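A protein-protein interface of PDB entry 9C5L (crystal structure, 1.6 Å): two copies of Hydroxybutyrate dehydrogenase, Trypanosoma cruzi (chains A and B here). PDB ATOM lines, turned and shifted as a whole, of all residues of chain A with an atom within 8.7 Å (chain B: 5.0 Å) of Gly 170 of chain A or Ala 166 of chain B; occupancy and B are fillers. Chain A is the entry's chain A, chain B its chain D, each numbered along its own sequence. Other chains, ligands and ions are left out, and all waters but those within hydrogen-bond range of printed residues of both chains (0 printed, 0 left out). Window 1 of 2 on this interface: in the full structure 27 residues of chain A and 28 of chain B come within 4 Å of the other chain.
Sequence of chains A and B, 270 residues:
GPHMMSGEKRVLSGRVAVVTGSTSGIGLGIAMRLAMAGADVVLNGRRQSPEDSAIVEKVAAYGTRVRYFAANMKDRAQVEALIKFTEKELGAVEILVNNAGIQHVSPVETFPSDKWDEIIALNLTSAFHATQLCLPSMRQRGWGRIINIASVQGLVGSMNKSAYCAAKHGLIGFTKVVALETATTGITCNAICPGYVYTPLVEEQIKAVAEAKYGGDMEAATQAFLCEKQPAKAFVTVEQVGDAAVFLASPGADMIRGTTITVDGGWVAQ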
ATOM      1  N   ILE A 120     -17.678  -6.244 -35.274  1.00  0.00           N
ATOM      2  CA  ILE A 120     -18.054  -5.705 -33.970  1.00  0.00           C
ATOM      3  C   ILE A 120     -19.186  -4.703 -34.140  1.00  0.00           C
ATOM      4  O   ILE A 120     -20.156  -4.703 -33.377  1.00  0.00           O
ATOM      5  CB  ILE A 120     -16.847  -5.070 -33.259  1.00  0.00           C
ATOM      6  CG1 ILE A 120     -15.761  -6.113 -33.005  1.00  0.00           C
ATOM      7  CG2 ILE A 120     -17.309  -4.421 -31.962  1.00  0.00           C
ATOM      8  CD1 ILE A 120     -16.193  -7.350 -32.298  1.00  0.00           C
ATOM      9  N   ASN A 123     -22.539  -6.824 -35.506  1.00  0.00           N
ATOM     10  CA  ASN A 123     -23.054  -7.924 -34.722  1.00  0.00           C
ATOM     11  C   ASN A 123     -23.223  -7.571 -33.240  1.00  0.00           C
ATOM     12  O   ASN A 123     -23.875  -8.332 -32.508  1.00  0.00           O
ATOM     13  CB  ASN A 123     -22.117  -9.131 -34.858  1.00  0.00           C
ATOM     14  CG  ASN A 123     -22.002  -9.640 -36.296  1.00  0.00           C
ATOM     15  OD1 ASN A 123     -22.409  -8.970 -37.244  1.00  0.00           O
ATOM     16  ND2 ASN A 123     -21.420 -10.801 -36.464  1.00  0.00           N
ATOM     17  N   LEU A 124     -22.599  -6.487 -32.756  1.00  0.00           N
ATOM     18  CA  LEU A 124     -22.758  -6.064 -31.364  1.00  0.00           C
ATOM     19  C   LEU A 124     -23.260  -4.631 -31.237  1.00  0.00           C
ATOM     20  O   LEU A 124     -24.331  -4.399 -30.666  1.00  0.00           O
ATOM     21  CB  LEU A 124     -21.419  -6.219 -30.631  1.00  0.00           C
ATOM     22  CG  LEU A 124     -21.331  -5.638 -29.208  1.00  0.00           C
ATOM     23  CD1 LEU A 124     -22.397  -6.255 -28.320  1.00  0.00           C
ATOM     24  CD2 LEU A 124     -19.939  -5.847 -28.663  1.00  0.00           C
ATOM     25  N   THR A 125     -22.534  -3.664 -31.777  1.00  0.00           N
ATOM     26  CA  THR A 125     -22.861  -2.266 -31.479  1.00  0.00           C
ATOM     27  C   THR A 125     -24.206  -1.845 -32.075  1.00  0.00           C
ATOM     28  O   THR A 125     -24.905  -1.009 -31.495  1.00  0.00           O
ATOM     29  CB  THR A 125     -21.719  -1.362 -31.960  1.00  0.00           C
ATOM     30  OG1 THR A 125     -20.531  -1.719 -31.215  1.00  0.00           O
ATOM     31  CG2 THR A 125     -22.034   0.115 -31.724  1.00  0.00           C
ATOM     32  N   ALA A 127     -26.904  -3.552 -32.250  1.00  0.00           N
ATOM     33  CA  ALA A 127     -27.948  -3.975 -31.331  1.00  0.00           C
ATOM     34  C   ALA A 127     -28.056  -2.994 -30.167  1.00  0.00           C
ATOM     35  O   ALA A 127     -29.153  -2.690 -29.694  1.00  0.00           O
ATOM     36  CB  ALA A 127     -27.655  -5.391 -30.826  1.00  0.00           C
ATOM     37  N   PHE A 128     -26.916  -2.503 -29.676  1.00  0.00           N
ATOM     38  CA  PHE A 128     -26.938  -1.486 -28.625  1.00  0.00           C
ATOM     39  C   PHE A 128     -27.682  -0.242 -29.104  1.00  0.00           C
ATOM     40  O   PHE A 128     -28.549   0.290 -28.397  1.00  0.00           O
ATOM     41  CB  PHE A 128     -25.502  -1.154 -28.209  1.00  0.00           C
ATOM     42  CG  PHE A 128     -25.336   0.178 -27.551  1.00  0.00           C
ATOM     43  CD1 PHE A 128     -25.953   0.474 -26.349  1.00  0.00           C
ATOM     44  CD2 PHE A 128     -24.507   1.131 -28.114  1.00  0.00           C
ATOM     45  CE1 PHE A 128     -25.776   1.729 -25.756  1.00  0.00           C
ATOM     46  CE2 PHE A 128     -24.313   2.359 -27.532  1.00  0.00           C
ATOM     47  CZ  PHE A 128     -24.944   2.664 -26.333  1.00  0.00           C
ATOM     48  N   ASN A 148     -32.178 -10.752 -29.115  1.00  0.00           N
ATOM     49  CA  ASN A 148     -30.883 -10.638 -29.780  1.00  0.00           C
ATOM     50  C   ASN A 148     -30.501 -11.982 -30.376  1.00  0.00           C
ATOM     51  O   ASN A 148     -30.497 -12.991 -29.668  1.00  0.00           O
ATOM     52  CB  ASN A 148     -29.842 -10.153 -28.774  1.00  0.00           C
ATOM     53  CG  ASN A 148     -30.128  -8.755 -28.302  1.00  0.00           C
ATOM     54  OD1 ASN A 148     -30.552  -7.927 -29.093  1.00  0.00           O
ATOM     55  ND2 ASN A 148     -29.933  -8.489 -27.014  1.00  0.00           N
ATOM     56  N   ALA A 150     -27.845 -14.082 -31.207  1.00  0.00           N
ATOM     57  CA  ALA A 150     -26.461 -14.419 -30.904  1.00  0.00           C
ATOM     58  C   ALA A 150     -26.115 -15.668 -31.718  1.00  0.00           C
ATOM     59  O   ALA A 150     -26.375 -15.711 -32.940  1.00  0.00           O
ATOM     60  CB  ALA A 150     -26.279 -14.558 -29.404  1.00  0.00           C
ATOM     61  N   GLN A 153     -21.513 -19.455 -31.026  1.00  0.00           N
ATOM     62  CA  GLN A 153     -20.220 -18.769 -30.994  1.00  0.00           C
ATOM     63  C   GLN A 153     -20.185 -17.635 -29.974  1.00  0.00           C
ATOM     64  O   GLN A 153     -19.125 -17.052 -29.760  1.00  0.00           O
ATOM     65  CB  GLN A 153     -19.859 -18.227 -32.399  1.00  0.00           C
ATOM     66  CG  GLN A 153     -19.948 -19.202 -33.559  1.00  0.00           C
ATOM     67  CD  GLN A 153     -18.880 -20.276 -33.557  1.00  0.00           C
ATOM     68  OE1 GLN A 153     -18.166 -20.437 -32.588  1.00  0.00           O
ATOM     69  NE2 GLN A 153     -18.780 -21.021 -34.659  1.00  0.00           N
ATOM     70  N   GLY A 154     -21.308 -17.306 -29.351  1.00  0.00           N
ATOM     71  CA  GLY A 154     -21.374 -16.446 -28.193  1.00  0.00           C
ATOM     72  C   GLY A 154     -21.193 -17.145 -26.873  1.00  0.00           C
ATOM     73  O   GLY A 154     -21.103 -16.462 -25.822  1.00  0.00           O
ATOM     74  N   LEU A 155     -21.155 -18.487 -26.905  1.00  0.00           N
ATOM     75  CA  LEU A 155     -20.984 -19.288 -25.702  1.00  0.00           C
ATOM     76  C   LEU A 155     -19.703 -20.104 -25.694  1.00  0.00           C
ATOM     77  O   LEU A 155     -19.198 -20.449 -24.599  1.00  0.00           O
ATOM     78  CB  LEU A 155     -22.174 -20.223 -25.526  1.00  0.00           C
ATOM     79  CG  LEU A 155     -23.524 -19.534 -25.315  1.00  0.00           C
ATOM     80  CD1 LEU A 155     -24.673 -20.533 -25.427  1.00  0.00           C
ATOM     81  CD2 LEU A 155     -23.573 -18.798 -23.978  1.00  0.00           C
ATOM     82  N   ALA A 163     -13.265 -12.529 -34.453  1.00  0.00           N
ATOM     83  CA  ALA A 163     -14.108 -11.335 -34.365  1.00  0.00           C
ATOM     84  C   ALA A 163     -15.555 -11.712 -34.072  1.00  0.00           C
ATOM     85  O   ALA A 163     -16.215 -11.077 -33.243  1.00  0.00           O
ATOM     86  CB  ALA A 163     -14.030 -10.526 -35.660  1.00  0.00           C
ATOM     87  N   TYR A 164     -16.073 -12.719 -34.785  1.00  0.00           N
ATOM     88  CA  TYR A 164     -17.465 -13.141 -34.633  1.00  0.00           C
ATOM     89  C   TYR A 164     -17.739 -13.730 -33.243  1.00  0.00           C
ATOM     90  O   TYR A 164     -18.735 -13.371 -32.609  1.00  0.00           O
ATOM     91  CB  TYR A 164     -17.764 -14.142 -35.729  1.00  0.00           C
ATOM     92  CG  TYR A 164     -19.177 -14.610 -35.877  1.00  0.00           C
ATOM     93  CD1 TYR A 164     -20.041 -14.000 -36.766  1.00  0.00           C
ATOM     94  CD2 TYR A 164     -19.621 -15.722 -35.194  1.00  0.00           C
ATOM     95  CE1 TYR A 164     -21.320 -14.461 -36.939  1.00  0.00           C
ATOM     96  CE2 TYR A 164     -20.903 -16.205 -35.370  1.00  0.00           C
ATOM     97  CZ  TYR A 164     -21.744 -15.579 -36.248  1.00  0.00           C
ATOM     98  OH  TYR A 164     -23.010 -16.053 -36.445  1.00  0.00           O
ATOM     99  N   CYS A 165     -16.849 -14.594 -32.727  1.00  0.00           N
ATOM    100  CA  CYS A 165     -17.017 -15.092 -31.376  1.00  0.00           C
ATOM    101  C   CYS A 165     -16.974 -13.953 -30.358  1.00  0.00           C
ATOM    102  O   CYS A 165     -17.740 -13.933 -29.385  1.00  0.00           O
ATOM    103  CB  CYS A 165     -15.946 -16.150 -31.057  1.00  0.00           C
ATOM    104  SG  CYS A 165     -16.199 -17.710 -31.951  1.00  0.00           S
ATOM    105  N   ALA A 166     -16.072 -12.989 -30.551  1.00  0.00           N
ATOM    106  CA  ALA A 166     -16.003 -11.870 -29.618  1.00  0.00           C
ATOM    107  C   ALA A 166     -17.306 -11.076 -29.658  1.00  0.00           C
ATOM    108  O   ALA A 166     -17.881 -10.750 -28.618  1.00  0.00           O
ATOM    109  CB  ALA A 166     -14.813 -10.964 -29.953  1.00  0.00           C
ATOM    110  N   ALA A 167     -17.803 -10.802 -30.858  1.00  0.00           N
ATOM    111  CA  ALA A 167     -19.015  -9.996 -31.001  1.00  0.00           C
ATOM    112  C   ALA A 167     -20.230 -10.703 -30.417  1.00  0.00           C
ATOM    113  O   ALA A 167     -21.053 -10.074 -29.726  1.00  0.00           O
ATOM    114  CB  ALA A 167     -19.237  -9.666 -32.477  1.00  0.00           C
ATOM    115  N   LYS A 168     -20.340 -12.013 -30.645  1.00  0.00           N
ATOM    116  CA  LYS A 168     -21.510 -12.751 -30.189  1.00  0.00           C
ATOM    117  C   LYS A 168     -21.469 -12.942 -28.667  1.00  0.00           C
ATOM    118  O   LYS A 168     -22.527 -12.907 -28.016  1.00  0.00           O
ATOM    119  CB  LYS A 168     -21.618 -14.079 -30.924  1.00  0.00           C
ATOM    120  CG  LYS A 168     -21.940 -13.969 -32.407  1.00  0.00           C
ATOM    121  CD  LYS A 168     -23.294 -13.323 -32.648  1.00  0.00           C
ATOM    122  CE  LYS A 168     -23.730 -13.505 -34.137  1.00  0.00           C
ATOM    123  NZ  LYS A 168     -24.975 -12.757 -34.430  1.00  0.00           N
ATOM    124  N   HIS A 169     -20.277 -13.237 -28.097  1.00  0.00           N
ATOM    125  CA  HIS A 169     -20.123 -13.220 -26.650  1.00  0.00           C
ATOM    126  C   HIS A 169     -20.570 -11.869 -26.097  1.00  0.00           C
ATOM    127  O   HIS A 169     -21.319 -11.781 -25.104  1.00  0.00           O
ATOM    128  CB  HIS A 169     -18.660 -13.501 -26.234  1.00  0.00           C
ATOM    129  CG  HIS A 169     -18.320 -14.961 -26.123  1.00  0.00           C
ATOM    130  ND1 HIS A 169     -18.182 -15.785 -27.221  1.00  0.00           N
ATOM    131  CD2 HIS A 169     -18.025 -15.731 -25.054  1.00  0.00           C
ATOM    132  CE1 HIS A 169     -17.896 -17.013 -26.828  1.00  0.00           C
ATOM    133  NE2 HIS A 169     -17.756 -17.006 -25.522  1.00  0.00           N
ATOM    134  N   GLY A 170     -20.102 -10.788 -26.728  1.00  0.00           N
ATOM    135  CA  GLY A 170     -20.457  -9.454 -26.261  1.00  0.00           C
ATOM    136  C   GLY A 170     -21.952  -9.215 -26.308  1.00  0.00           C
ATOM    137  O   GLY A 170     -22.501  -8.543 -25.434  1.00  0.00           O
ATOM    138  N   LEU A 171     -22.608  -9.704 -27.350  1.00  0.00           N
ATOM    139  CA  LEU A 171     -24.058  -9.521 -27.486  1.00  0.00           C
ATOM    140  C   LEU A 171     -24.809 -10.247 -26.372  1.00  0.00           C
ATOM    141  O   LEU A 171     -25.830  -9.741 -25.858  1.00  0.00           O
ATOM    142  CB  LEU A 171     -24.526  -9.980 -28.867  1.00  0.00           C
ATOM    143  CG  LEU A 171     -25.992  -9.793 -29.169  1.00  0.00           C
ATOM    144  CD1 LEU A 171     -26.357  -8.319 -29.228  1.00  0.00           C
ATOM    145  CD2 LEU A 171     -26.295 -10.475 -30.529  1.00  0.00           C
ATOM    146  N   ILE A 172     -24.300 -11.396 -25.950  1.00  0.00           N
ATOM    147  CA  ILE A 172     -24.899 -12.103 -24.821  1.00  0.00           C
ATOM    148  C   ILE A 172     -24.688 -11.313 -23.514  1.00  0.00           C
ATOM    149  O   ILE A 172     -25.612 -11.176 -22.693  1.00  0.00           O
ATOM    150  CB  ILE A 172     -24.340 -13.540 -24.771  1.00  0.00           C
ATOM    151  CG1 ILE A 172     -24.869 -14.349 -25.950  1.00  0.00           C
ATOM    152  CG2 ILE A 172     -24.655 -14.235 -23.441  1.00  0.00           C
ATOM    153  CD1 ILE A 172     -24.349 -15.753 -26.053  1.00  0.00           C
ATOM    154  N   GLY A 173     -23.484 -10.744 -23.305  1.00  0.00           N
ATOM    155  CA  GLY A 173     -23.276  -9.911 -22.116  1.00  0.00           C
ATOM    156  C   GLY A 173     -24.209  -8.710 -22.098  1.00  0.00           C
ATOM    157  O   GLY A 173     -24.785  -8.359 -21.058  1.00  0.00           O
ATOM    158  N   PHE A 174     -24.338  -8.058 -23.250  1.00  0.00           N
ATOM    159  CA  PHE A 174     -25.258  -6.923 -23.388  1.00  0.00           C
ATOM    160  C   PHE A 174     -26.687  -7.324 -23.053  1.00  0.00           C
ATOM    161  O   PHE A 174     -27.400  -6.589 -22.344  1.00  0.00           O
ATOM    162  CB  PHE A 174     -25.168  -6.355 -24.811  1.00  0.00           C
ATOM    163  CG  PHE A 174     -26.123  -5.220 -25.063  1.00  0.00           C
ATOM    164  CD1 PHE A 174     -25.919  -3.997 -24.473  1.00  0.00           C
ATOM    165  CD2 PHE A 174     -27.186  -5.377 -25.937  1.00  0.00           C
ATOM    166  CE1 PHE A 174     -26.784  -2.939 -24.685  1.00  0.00           C
ATOM    167  CE2 PHE A 174     -28.048  -4.315 -26.155  1.00  0.00           C
ATOM    168  CZ  PHE A 174     -27.839  -3.112 -25.513  1.00  0.00           C
ATOM    169  N   THR A 175     -27.104  -8.489 -23.530  1.00  0.00           N
ATOM    170  CA  THR A 175     -28.438  -9.010 -23.240  1.00  0.00           C
ATOM    171  C   THR A 175     -28.680  -9.108 -21.736  1.00  0.00           C
ATOM    172  O   THR A 175     -29.736  -8.698 -21.235  1.00  0.00           O
ATOM    173  CB  THR A 175     -28.583 -10.379 -23.871  1.00  0.00           C
ATOM    174  OG1 THR A 175     -28.483 -10.288 -25.312  1.00  0.00           O
ATOM    175  CG2 THR A 175     -29.912 -11.037 -23.485  1.00  0.00           C
ATOM    176  N   LYS A 176     -27.717  -9.680 -21.009  1.00  0.00           N
ATOM    177  CA  LYS A 176     -27.847  -9.791 -19.557  1.00  0.00           C
ATOM    178  C   LYS A 176     -28.079  -8.422 -18.928  1.00  0.00           C
ATOM    179  O   LYS A 176     -28.943  -8.269 -18.051  1.00  0.00           O
ATOM    180  CB  LYS A 176     -26.598 -10.453 -18.959  1.00  0.00           C
ATOM    181  CG  LYS A 176     -26.438 -11.882 -19.451  1.00  0.00           C
ATOM    182  CD  LYS A 176     -25.139 -12.485 -18.929  1.00  0.00           C
ATOM    183  CE  LYS A 176     -24.783 -13.719 -19.699  1.00  0.00           C
ATOM    184  NZ  LYS A 176     -23.466 -14.300 -19.326  1.00  0.00           N
ATOM    185  N   VAL A 177     -27.271  -7.421 -19.315  1.00  0.00           N
ATOM    186  CA  VAL A 177     -27.380  -6.118 -18.662  1.00  0.00           C
ATOM    187  C   VAL A 177     -28.740  -5.488 -18.960  1.00  0.00           C
ATOM    188  O   VAL A 177     -29.426  -5.005 -18.050  1.00  0.00           O
ATOM    189  CB  VAL A 177     -26.237  -5.184 -19.093  1.00  0.00           C
ATOM    190  CG1 VAL A 177     -26.440  -3.791 -18.482  1.00  0.00           C
ATOM    191  CG2 VAL A 177     -24.908  -5.762 -18.647  1.00  0.00           C
ATOM    192  N   ALA A 191     -31.469 -13.657 -25.577  1.00  0.00           N
ATOM    193  CA  ALA A 191     -30.776 -13.988 -26.814  1.00  0.00           C
ATOM    194  C   ALA A 191     -31.153 -15.392 -27.250  1.00  0.00           C
ATOM    195  O   ALA A 191     -31.362 -16.294 -26.430  1.00  0.00           O
ATOM    196  CB  ALA A 191     -29.247 -13.901 -26.606  1.00  0.00           C
ATOM    197  N   TRP B 116     -19.399   4.112 -25.157  1.00  0.00           N
ATOM    198  CA  TRP B 116     -19.539   2.736 -25.635  1.00  0.00           C
ATOM    199  C   TRP B 116     -18.379   2.376 -26.559  1.00  0.00           C
ATOM    200  O   TRP B 116     -17.699   1.347 -26.365  1.00  0.00           O
ATOM    201  CB  TRP B 116     -20.888   2.561 -26.353  1.00  0.00           C
ATOM    202  CG  TRP B 116     -21.053   1.184 -26.977  1.00  0.00           C
ATOM    203  CD1 TRP B 116     -20.554   0.779 -28.184  1.00  0.00           C
ATOM    204  CD2 TRP B 116     -21.754   0.058 -26.433  1.00  0.00           C
ATOM    205  NE1 TRP B 116     -20.890  -0.528 -28.414  1.00  0.00           N
ATOM    206  CE2 TRP B 116     -21.634  -0.998 -27.365  1.00  0.00           C
ATOM    207  CE3 TRP B 116     -22.484  -0.161 -25.262  1.00  0.00           C
ATOM    208  CZ2 TRP B 116     -22.199  -2.252 -27.146  1.00  0.00           C
ATOM    209  CZ3 TRP B 116     -23.065  -1.373 -25.061  1.00  0.00           C
ATOM    210  CH2 TRP B 116     -22.897  -2.432 -25.987  1.00  0.00           C
ATOM    211  N   ILE B 120     -15.408  -0.506 -25.948  1.00  0.00           N
ATOM    212  CA  ILE B 120     -15.171  -1.618 -26.871  1.00  0.00           C
ATOM    213  C   ILE B 120     -13.737  -1.558 -27.398  1.00  0.00           C
ATOM    214  O   ILE B 120     -13.046  -2.584 -27.493  1.00  0.00           O
ATOM    215  CB  ILE B 120     -16.188  -1.592 -28.031  1.00  0.00           C
ATOM    216  CG1 ILE B 120     -17.633  -1.728 -27.526  1.00  0.00           C
ATOM    217  CG2 ILE B 120     -15.875  -2.721 -29.032  1.00  0.00           C
ATOM    218  CD1 ILE B 120     -17.899  -2.902 -26.690  1.00  0.00           C
ATOM    219  N   LYS B 161     -23.788  -1.290 -16.636  1.00  0.00           N
ATOM    220  CA  LYS B 161     -22.474  -1.570 -17.176  1.00  0.00           C
ATOM    221  C   LYS B 161     -22.582  -2.293 -18.513  1.00  0.00           C
ATOM    222  O   LYS B 161     -21.832  -3.229 -18.807  1.00  0.00           O
ATOM    223  CB  LYS B 161     -21.649  -2.356 -16.159  1.00  0.00           C
ATOM    224  CG  LYS B 161     -21.315  -1.508 -14.921  1.00  0.00           C
ATOM    225  CD  LYS B 161     -20.530  -2.325 -13.872  1.00  0.00           C
ATOM    226  CE  LYS B 161     -20.099  -1.366 -12.770  1.00  0.00           C
ATOM    227  NZ  LYS B 161     -19.445  -2.134 -11.626  1.00  0.00           N
ATOM    228  N   SER B 162     -23.503  -1.843 -19.369  1.00  0.00           N
ATOM    229  CA  SER B 162     -23.741  -2.571 -20.619  1.00  0.00           C
ATOM    230  C   SER B 162     -22.484  -2.655 -21.484  1.00  0.00           C
ATOM    231  O   SER B 162     -22.134  -3.733 -21.994  1.00  0.00           O
ATOM    232  CB  SER B 162     -24.897  -1.906 -21.376  1.00  0.00           C
ATOM    233  OG  SER B 162     -24.645  -0.532 -21.650  1.00  0.00           O
ATOM    234  N   ALA B 163     -21.825  -1.519 -21.727  1.00  0.00           N
ATOM    235  CA  ALA B 163     -20.657  -1.536 -22.603  1.00  0.00           C
ATOM    236  C   ALA B 163     -19.559  -2.413 -22.019  1.00  0.00           C
ATOM    237  O   ALA B 163     -18.917  -3.181 -22.740  1.00  0.00           O
ATOM    238  CB  ALA B 163     -20.123  -0.132 -22.805  1.00  0.00           C
ATOM    239  N   TYR B 164     -19.306  -2.274 -20.716  1.00  0.00           N
ATOM    240  CA  TYR B 164     -18.220  -3.012 -20.082  1.00  0.00           C
ATOM    241  C   TYR B 164     -18.493  -4.502 -20.074  1.00  0.00           C
ATOM    242  O   TYR B 164     -17.601  -5.303 -20.377  1.00  0.00           O
ATOM    243  CB  TYR B 164     -18.041  -2.474 -18.668  1.00  0.00           C
ATOM    244  CG  TYR B 164     -16.878  -3.006 -17.871  1.00  0.00           C
ATOM    245  CD1 TYR B 164     -17.037  -4.073 -17.025  1.00  0.00           C
ATOM    246  CD2 TYR B 164     -15.666  -2.336 -17.861  1.00  0.00           C
ATOM    247  CE1 TYR B 164     -16.003  -4.507 -16.231  1.00  0.00           C
ATOM    248  CE2 TYR B 164     -14.614  -2.766 -17.067  1.00  0.00           C
ATOM    249  CZ  TYR B 164     -14.798  -3.853 -16.265  1.00  0.00           C
ATOM    250  OH  TYR B 164     -13.754  -4.272 -15.478  1.00  0.00           O
ATOM    251  N   CYS B 165     -19.712  -4.902 -19.724  1.00  0.00           N
ATOM    252  CA  CYS B 165     -20.072  -6.306 -19.747  1.00  0.00           C
ATOM    253  C   CYS B 165     -19.979  -6.858 -21.167  1.00  0.00           C
ATOM    254  O   CYS B 165     -19.511  -7.983 -21.378  1.00  0.00           O
ATOM    255  CB  CYS B 165     -21.483  -6.502 -19.199  1.00  0.00           C
ATOM    256  SG  CYS B 165     -21.590  -6.287 -17.425  1.00  0.00           S
ATOM    257  N   ALA B 166     -20.416  -6.083 -22.161  1.00  0.00           N
ATOM    258  CA  ALA B 166     -20.290  -6.561 -23.532  1.00  0.00           C
ATOM    259  C   ALA B 166     -18.830  -6.746 -23.915  1.00  0.00           C
ATOM    260  O   ALA B 166     -18.460  -7.782 -24.490  1.00  0.00           O
ATOM    261  CB  ALA B 166     -20.984  -5.587 -24.483  1.00  0.00           C
ATOM    262  N   ALA B 167     -17.988  -5.764 -23.600  1.00  0.00           N
ATOM    263  CA  ALA B 167     -16.580  -5.833 -23.980  1.00  0.00           C
ATOM    264  C   ALA B 167     -15.858  -6.974 -23.269  1.00  0.00           C
ATOM    265  O   ALA B 167     -15.065  -7.687 -23.885  1.00  0.00           O
ATOM    266  CB  ALA B 167     -15.888  -4.494 -23.691  1.00  0.00           C
ATOM    267  N   LYS B 168     -16.141  -7.179 -21.981  1.00  0.00           N
ATOM    268  CA  LYS B 168     -15.479  -8.252 -21.228  1.00  0.00           C
ATOM    269  C   LYS B 168     -15.958  -9.633 -21.670  1.00  0.00           C
ATOM    270  O   LYS B 168     -15.151 -10.577 -21.778  1.00  0.00           O
ATOM    271  CB  LYS B 168     -15.702  -8.027 -19.733  1.00  0.00           C
ATOM    272  CG  LYS B 168     -15.011  -6.777 -19.211  1.00  0.00           C
ATOM    273  CD  LYS B 168     -13.496  -6.870 -19.321  1.00  0.00           C
ATOM    274  CE  LYS B 168     -12.822  -5.691 -18.560  1.00  0.00           C
ATOM    275  NZ  LYS B 168     -11.344  -5.802 -18.572  1.00  0.00           N
ATOM    276  N   HIS B 169     -17.273  -9.793 -21.921  1.00  0.00           N
ATOM    277  CA  HIS B 169     -17.766 -11.029 -22.532  1.00  0.00           C
ATOM    278  C   HIS B 169     -17.040 -11.278 -23.869  1.00  0.00           C
ATOM    279  O   HIS B 169     -16.526 -12.379 -24.137  1.00  0.00           O
ATOM    280  CB  HIS B 169     -19.287 -10.948 -22.772  1.00  0.00           C
ATOM    281  CG  HIS B 169     -20.141 -11.360 -21.626  1.00  0.00           C
ATOM    282  ND1 HIS B 169     -20.257 -10.607 -20.467  1.00  0.00           N
ATOM    283  CD2 HIS B 169     -20.958 -12.431 -21.458  1.00  0.00           C
ATOM    284  CE1 HIS B 169     -21.121 -11.195 -19.655  1.00  0.00           C
ATOM    285  NE2 HIS B 169     -21.542 -12.306 -20.220  1.00  0.00           N
ATOM    286  N   GLY B 170     -16.885 -10.229 -24.685  1.00  0.00           N
ATOM    287  CA  GLY B 170     -16.216 -10.391 -25.972  1.00  0.00           C
ATOM    288  C   GLY B 170     -14.754 -10.781 -25.830  1.00  0.00           C
ATOM    289  O   GLY B 170     -14.239 -11.569 -26.625  1.00  0.00           O
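Of the 12 printed residues of chain B, 8 touch a printed residue of chain A.
Printed residues of chain B that touch a printed residue of chain A: Trp 116, Ile 120, Lys 161, Ser 162, Cys 165, Ala 166, His 169 and Gly 170.
Among the printed residues, 16 pairs touch across the chains.
The side-chain hydroxyl (OG1) of Thr 125 of chain A sits at hydrogen-bond distance from the indole nitrogen (NE1) of Trp 116 of chain B.
The side-chain amino group (NZ) of Lys 176 of chain A lies within hydrogen-bond range of a ring nitrogen (NE2) of His 169 of chain B, 2.9 Å away.
Ala 150 of chain A touches none of the printed residues of chain B.
Of the printed residues of chain B, His 169 of chain A touches His 169 (3.2 Å) and Gly 170 (3.96 Å).
Gly 170 of chain A touches three residues of chain B.
Of the printed residues of chain B, Lys 176 of chain A touches His 169 (2.9 Å).
Of the printed residues of chain A, Ile 120 of chain B touches Ile 120 (3.7 Å).
Of the printed residues of chain A, Ser 162 of chain B touches Phe 174 (3.9 Å) and Val 177 (3.6 Å).
Of the printed residues of chain A, Cys 165 of chain B touches Val 177 (3.5 Å).
Of the printed residues of chain A, Ala 166 of chain B touches Gly 170 (3.1 Å).
No residue of chain A comes within 4 Å of Ala 167 of chain B.
The nearest residue of chain A that does not touch Ala 166 of chain B is Leu 124 of chain A (4.1 Å).
The nearest printed residue of chain B that does not touch Ala 166 of chain A is His 169 of chain B (4.9 Å).
Ile 120 of chain A touches its own counterpart, Ile 120 of chain B.
Ala 166 of chain A touches Gly 170 of chain B, and with the chains exchanged Gly 170 of chain A touches Ala 166 of chain B.
His 169 of chain B touches its own counterpart, His 169 of chain A.
Gly 170 of chain B touches its own counterpart, Gly 170 of chain A.
Positions printed for both chains: 120, 163, 164, 165, 166, 167, 168, 169 and 170.
Of the 16 pairs that touch across the chains among the printed residues, 7 have their exchanged pair printed and touching as well.
The backbone carbonyl oxygen of Ile 120 of chain A lies within hydrogen-bond range of the backbone NH of Thr 125 of chain A (3.0 Å).
The backbone carbonyl oxygen (O) of Gln 153 of chain A sits at hydrogen-bond distance from a ring nitrogen (ND1) of His 169 of chain A.
O of Gly 154 of chain A sits close to ND1 of His 169 of chain A, 3.3 Å away.
The backbone carbonyl oxygen (O) of Cys 165 of chain A sits at hydrogen-bond distance from a ring nitrogen (ND1) of His 169 of chain A, 2.9 Å away.
The side-chain sulfur (SG) of Cys 165 of chain B lies close to the backbone carbonyl oxygen (O) of Lys 161 of chain B.
The backbone carbonyl oxygen of Cys 165 of chain B lies within hydrogen-bond range of a ring nitrogen (ND1) of His 169 of chain B (2.9 Å).
Among the printed residues, merely in contact across the chains: Ala 166 of chain A with Gly 170 of chain B (3.1 Å), Gly 170 of chain A with Ala 166 of chain B (3.1 Å), His 169 of chain A with His 169 of chain B (3.2 Å), Phe 128 of chain A with Trp 116 of chain B (3.4 Å), Gly 173 of chain A with His 169 of chain B (3.5 Å), Val 177 of chain A with Cys 165 of chain B (3.5 Å), Val 177 of chain A with Ser 162 of chain B (3.6 Å), Ile 120 of chain A with Ile 120 of chain B (3.7 Å), Phe 174 of chain A with Trp 116 of chain B (3.7 Å), Gly 170 of chain A with Gly 170 of chain B (3.9 Å), Phe 174 of chain A with Ser 162 of chain B (3.9 Å), His 169 of chain A with Gly 170 of chain B (3.96 Å), Gly 170 of chain A with His 169 of chain B (3.97 Å) and Val 177 of chain A with Lys 161 of chain B (3.99 Å).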
